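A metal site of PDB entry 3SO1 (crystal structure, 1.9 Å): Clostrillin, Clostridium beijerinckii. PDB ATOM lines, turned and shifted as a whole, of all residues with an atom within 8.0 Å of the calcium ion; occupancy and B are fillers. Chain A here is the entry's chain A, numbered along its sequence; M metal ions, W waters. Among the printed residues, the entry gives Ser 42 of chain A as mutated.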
ATOM      1  N   TYR A   9     -29.150 -25.656 -16.247  1.00  0.00           N
ATOM      2  CA  TYR A   9     -28.372 -25.685 -17.489  1.00  0.00           C
ATOM      3  C   TYR A   9     -27.228 -24.673 -17.528  1.00  0.00           C
ATOM      4  O   TYR A   9     -27.356 -23.558 -17.011  1.00  0.00           O
ATOM      5  CB  TYR A   9     -29.283 -25.466 -18.701  1.00  0.00           C
ATOM      6  CG  TYR A   9     -30.287 -26.557 -18.936  1.00  0.00           C
ATOM      7  CD1 TYR A   9     -31.527 -26.536 -18.309  1.00  0.00           C
ATOM      8  CD2 TYR A   9     -30.003 -27.617 -19.808  1.00  0.00           C
ATOM      9  CE1 TYR A   9     -32.461 -27.536 -18.527  1.00  0.00           C
ATOM     10  CE2 TYR A   9     -30.933 -28.624 -20.031  1.00  0.00           C
ATOM     11  CZ  TYR A   9     -32.155 -28.574 -19.387  1.00  0.00           C
ATOM     12  OH  TYR A   9     -33.087 -29.565 -19.596  1.00  0.00           O
ATOM     13  N   GLU A  10     -26.139 -25.085 -18.160  1.00  0.00           N
ATOM     14  CA  GLU A  10     -24.937 -24.268 -18.324  1.00  0.00           C
ATOM     15  C   GLU A  10     -25.188 -23.029 -19.174  1.00  0.00           C
ATOM     16  O   GLU A  10     -24.743 -21.937 -18.826  1.00  0.00           O
ATOM     17  CB  GLU A  10     -23.829 -25.120 -18.941  1.00  0.00           C
ATOM     18  CG  GLU A  10     -22.500 -24.410 -19.149  1.00  0.00           C
ATOM     19  CD  GLU A  10     -21.471 -25.292 -19.842  1.00  0.00           C
ATOM     20  OE1 GLU A  10     -21.850 -26.381 -20.332  1.00  0.00           O
ATOM     21  OE2 GLU A  10     -20.293 -24.893 -19.904  1.00  0.00           O
ATOM     22  N   ASP A  11     -25.909 -23.200 -20.277  1.00  0.00           N
ATOM     23  CA  ASP A  11     -26.105 -22.121 -21.266  1.00  0.00           C
ATOM     24  C   ASP A  11     -27.553 -21.670 -21.355  1.00  0.00           C
ATOM     25  O   ASP A  11     -28.465 -22.379 -20.918  1.00  0.00           O
ATOM     26  CB  ASP A  11     -25.649 -22.572 -22.657  1.00  0.00           C
ATOM     27  CG  ASP A  11     -24.182 -22.978 -22.714  1.00  0.00           C
ATOM     28  OD1 ASP A  11     -23.354 -22.442 -21.940  1.00  0.00           O
ATOM     29  OD2 ASP A  11     -23.848 -23.831 -23.554  1.00  0.00           O
ATOM     30  N   ILE A  12     -27.759 -20.490 -21.931  1.00  0.00           N
ATOM     31  CA  ILE A  12     -29.083 -19.994 -22.312  1.00  0.00           C
ATOM     32  C   ILE A  12     -29.802 -21.030 -23.179  1.00  0.00           C
ATOM     33  O   ILE A  12     -29.155 -21.828 -23.868  1.00  0.00           O
ATOM     34  CB  ILE A  12     -28.975 -18.634 -23.062  1.00  0.00           C
ATOM     35  CG1 ILE A  12     -30.358 -17.993 -23.266  1.00  0.00           C
ATOM     36  CG2 ILE A  12     -28.197 -18.787 -24.386  1.00  0.00           C
ATOM     37  CD1 ILE A  12     -30.318 -16.541 -23.710  1.00  0.00           C
ATOM     38  N   GLY A  15     -29.015 -25.026 -22.981  1.00  0.00           N
ATOM     39  CA  GLY A  15     -27.840 -25.510 -23.706  1.00  0.00           C
ATOM     40  C   GLY A  15     -26.710 -25.943 -22.796  1.00  0.00           C
ATOM     41  O   GLY A  15     -26.699 -25.623 -21.602  1.00  0.00           O
ATOM     42  N   ASN A  38     -19.588 -23.431  -9.593  1.00  0.00           N
ATOM     43  CA  ASN A  38     -19.980 -22.080  -9.177  1.00  0.00           C
ATOM     44  C   ASN A  38     -20.111 -21.191 -10.393  1.00  0.00           C
ATOM     45  O   ASN A  38     -19.476 -21.445 -11.425  1.00  0.00           O
ATOM     46  CB  ASN A  38     -18.938 -21.496  -8.218  1.00  0.00           C
ATOM     47  CG  ASN A  38     -19.508 -20.402  -7.317  1.00  0.00           C
ATOM     48  OD1 ASN A  38     -20.667 -20.027  -7.416  1.00  0.00           O
ATOM     49  ND2 ASN A  38     -18.670 -19.886  -6.422  1.00  0.00           N
ATOM     50  N   ASP A  39     -20.961 -20.173 -10.291  1.00  0.00           N
ATOM     51  CA  ASP A  39     -21.109 -19.126 -11.307  1.00  0.00           C
ATOM     52  C   ASP A  39     -21.292 -19.670 -12.731  1.00  0.00           C
ATOM     53  O   ASP A  39     -20.526 -19.339 -13.636  1.00  0.00           O
ATOM     54  CB  ASP A  39     -19.905 -18.163 -11.234  1.00  0.00           C
ATOM     55  CG  ASP A  39     -19.813 -17.448  -9.889  1.00  0.00           C
ATOM     56  OD1 ASP A  39     -20.875 -17.216  -9.271  1.00  0.00           O
ATOM     57  OD2 ASP A  39     -18.687 -17.134  -9.469  1.00  0.00           O
ATOM     58  N   TRP A  40     -22.333 -20.482 -12.924  1.00  0.00           N
ATOM     59  CA  TRP A  40     -22.438 -21.372 -14.085  1.00  0.00           C
ATOM     60  C   TRP A  40     -23.849 -21.442 -14.659  1.00  0.00           C
ATOM     61  O   TRP A  40     -24.028 -21.509 -15.883  1.00  0.00           O
ATOM     62  CB  TRP A  40     -21.944 -22.753 -13.642  1.00  0.00           C
ATOM     63  CG  TRP A  40     -22.186 -23.946 -14.536  1.00  0.00           C
ATOM     64  CD1 TRP A  40     -21.324 -24.479 -15.462  1.00  0.00           C
ATOM     65  CD2 TRP A  40     -23.334 -24.816 -14.526  1.00  0.00           C
ATOM     66  NE1 TRP A  40     -21.871 -25.596 -16.038  1.00  0.00           N
ATOM     67  CE2 TRP A  40     -23.098 -25.835 -15.484  1.00  0.00           C
ATOM     68  CE3 TRP A  40     -24.531 -24.829 -13.806  1.00  0.00           C
ATOM     69  CZ2 TRP A  40     -24.028 -26.842 -15.748  1.00  0.00           C
ATOM     70  CZ3 TRP A  40     -25.462 -25.836 -14.071  1.00  0.00           C
ATOM     71  CH2 TRP A  40     -25.201 -26.827 -15.025  1.00  0.00           C
ATOM     72  N   MET A  41     -24.851 -21.439 -13.789  1.00  0.00           N
ATOM     73  CA  MET A  41     -26.243 -21.612 -14.190  1.00  0.00           C
ATOM     74  C   MET A  41     -26.746 -20.432 -15.042  1.00  0.00           C
ATOM     75  O   MET A  41     -26.652 -19.276 -14.629  1.00  0.00           O
ATOM     76  CB  MET A  41     -27.113 -21.806 -12.937  1.00  0.00           C
ATOM     77  CG  MET A  41     -28.489 -22.392 -13.205  1.00  0.00           C
ATOM     78  SD  MET A  41     -29.695 -21.141 -13.680  1.00  0.00           S
ATOM     79  CE  MET A  41     -30.108 -20.425 -12.086  1.00  0.00           C
ATOM     80  N   SER A  42     -27.277 -20.740 -16.223  1.00  0.00           N
ATOM     81  CA  SER A  42     -27.814 -19.718 -17.142  1.00  0.00           C
ATOM     82  C   SER A  42     -29.300 -19.929 -17.480  1.00  0.00           C
ATOM     83  O   SER A  42     -29.989 -18.982 -17.869  1.00  0.00           O
ATOM     84  CB  SER A  42     -26.999 -19.636 -18.426  1.00  0.00           C
ATOM     85  OG  SER A  42     -25.662 -19.227 -18.161  1.00  0.00           O
ATOM     86  N   SER A  43     -29.771 -21.162 -17.361  1.00  0.00           N
ATOM     87  CA  SER A  43     -31.191 -21.468 -17.533  1.00  0.00           C
ATOM     88  C   SER A  43     -31.579 -22.690 -16.715  1.00  0.00           C
ATOM     89  O   SER A  43     -30.713 -23.453 -16.278  1.00  0.00           O
ATOM     90  CB  SER A  43     -31.545 -21.641 -19.022  1.00  0.00           C
ATOM     91  OG  SER A  43     -30.827 -22.710 -19.628  1.00  0.00           O
ATOM     92  N   TRP A  73     -33.913 -18.256 -20.003  1.00  0.00           N
ATOM     93  CA  TRP A  73     -32.909 -17.229 -19.796  1.00  0.00           C
ATOM     94  C   TRP A  73     -33.165 -16.480 -18.482  1.00  0.00           C
ATOM     95  O   TRP A  73     -34.157 -15.764 -18.343  1.00  0.00           O
ATOM     96  CB  TRP A  73     -32.868 -16.255 -20.985  1.00  0.00           C
ATOM     97  CG  TRP A  73     -31.914 -15.090 -20.848  1.00  0.00           C
ATOM     98  CD1 TRP A  73     -32.202 -13.772 -21.096  1.00  0.00           C
ATOM     99  CD2 TRP A  73     -30.537 -15.133 -20.450  1.00  0.00           C
ATOM    100  NE1 TRP A  73     -31.096 -12.993 -20.873  1.00  0.00           N
ATOM    101  CE2 TRP A  73     -30.052 -13.800 -20.478  1.00  0.00           C
ATOM    102  CE3 TRP A  73     -29.657 -16.152 -20.070  1.00  0.00           C
ATOM    103  CZ2 TRP A  73     -28.734 -13.469 -20.137  1.00  0.00           C
ATOM    104  CZ3 TRP A  73     -28.347 -15.823 -19.733  1.00  0.00           C
ATOM    105  CH2 TRP A  73     -27.901 -14.494 -19.775  1.00  0.00           C
ATOM    106  N   VAL A  74     -32.270 -16.666 -17.517  1.00  0.00           N
ATOM    107  CA  VAL A  74     -32.405 -16.039 -16.207  1.00  0.00           C
ATOM    108  C   VAL A  74     -32.198 -14.515 -16.242  1.00  0.00           C
ATOM    109  O   VAL A  74     -32.603 -13.809 -15.320  1.00  0.00           O
ATOM    110  CB  VAL A  74     -31.471 -16.679 -15.126  1.00  0.00           C
ATOM    111  CG1 VAL A  74     -31.884 -18.120 -14.847  1.00  0.00           C
ATOM    112  CG2 VAL A  74     -30.014 -16.602 -15.538  1.00  0.00           C
ATOM    113  N   ASN A  79     -27.578 -14.310 -14.169  1.00  0.00           N
ATOM    114  CA  ASN A  79     -26.730 -15.216 -14.948  1.00  0.00           C
ATOM    115  C   ASN A  79     -25.390 -15.507 -14.302  1.00  0.00           C
ATOM    116  O   ASN A  79     -24.724 -14.606 -13.799  1.00  0.00           O
ATOM    117  CB  ASN A  79     -26.504 -14.670 -16.363  1.00  0.00           C
ATOM    118  CG  ASN A  79     -25.768 -15.653 -17.241  1.00  0.00           C
ATOM    119  OD1 ASN A  79     -26.201 -16.784 -17.417  1.00  0.00           O
ATOM    120  ND2 ASN A  79     -24.638 -15.220 -17.790  1.00  0.00           N
ATOM    121  N   ASP A  80     -25.004 -16.787 -14.318  1.00  0.00           N
ATOM    122  CA  ASP A  80     -23.722 -17.241 -13.777  1.00  0.00           C
ATOM    123  C   ASP A  80     -23.453 -16.706 -12.376  1.00  0.00           C
ATOM    124  O   ASP A  80     -22.361 -16.206 -12.102  1.00  0.00           O
ATOM    125  CB  ASP A  80     -22.561 -16.848 -14.704  1.00  0.00           C
ATOM    126  CG  ASP A  80     -22.578 -17.587 -16.021  1.00  0.00           C
ATOM    127  OD1 ASP A  80     -23.339 -18.564 -16.182  1.00  0.00           O
ATOM    128  OD2 ASP A  80     -21.801 -17.181 -16.924  1.00  0.00           O
ATOM    129  N   LYS A  81     -24.449 -16.793 -11.488  1.00  0.00           N
ATOM    130  CA  LYS A  81     -24.263 -16.324 -10.115  1.00  0.00           C
ATOM    131  C   LYS A  81     -24.692 -17.332  -9.040  1.00  0.00           C
ATOM    132  O   LYS A  81     -24.311 -17.198  -7.876  1.00  0.00           O
ATOM    133  CB  LYS A  81     -24.952 -14.979  -9.885  1.00  0.00           C
ATOM    134  CG  LYS A  81     -24.215 -13.797 -10.501  1.00  0.00           C
ATOM    135  CD  LYS A  81     -24.854 -12.486 -10.109  1.00  0.00           C
ATOM    136  CE  LYS A  81     -24.165 -11.309 -10.785  1.00  0.00           C
ATOM    137  NZ  LYS A  81     -24.986 -10.060 -10.649  1.00  0.00           N
HETATM  138 CA    CA M   1     -23.482 -20.206 -17.930  1.00  0.00          CA
HETATM  139  O   HOH W   1     -23.342 -20.173 -20.470  1.00  0.00           O
HETATM  140  O   HOH W   2     -21.243 -21.012 -17.708  1.00  0.00           O
HETATM  141  O   HOH W   3     -22.973 -18.081 -19.038  1.00  0.00           O
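OG of Ser 42 sits close to OD1 of Asn 79, 2.6 Å away.
The backbone NH (N) of Ser 42 is in hydrogen-bond range of the backbone carbonyl oxygen (O) of Tyr 9, 2.9 Å away.
The backbone NH of Val 74 is in hydrogen-bond range of the backbone carbonyl oxygen of Ser 42.
The backbone NH (N) of Asp 80 sits at hydrogen-bond distance from the backbone carbonyl oxygen (O) of Met 41 (3.0 Å).
Within 4 Å of the calcium ion: Glu 10, Trp 40, Ser 42 and Asp 80.
The nearest printed residue that does not touch the calcium ion is Met 41 (4.4 Å).
The calcium ion is bound by the backbone carbonyl oxygen (O) of Glu 10 (2.3 Å), water W2 (2.4 Å), the side-chain hydroxyl (OG) of Ser 42 (2.4 Å), the side-chain carboxylate (OD1) of Asp 80 (2.4 Å), water W3 (2.4 Å), the backbone carbonyl oxygen (O) of Trp 40 (2.5 Å) and water W1 (2.5 Å).
The calcium ion has seven donor atoms within binding distance.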
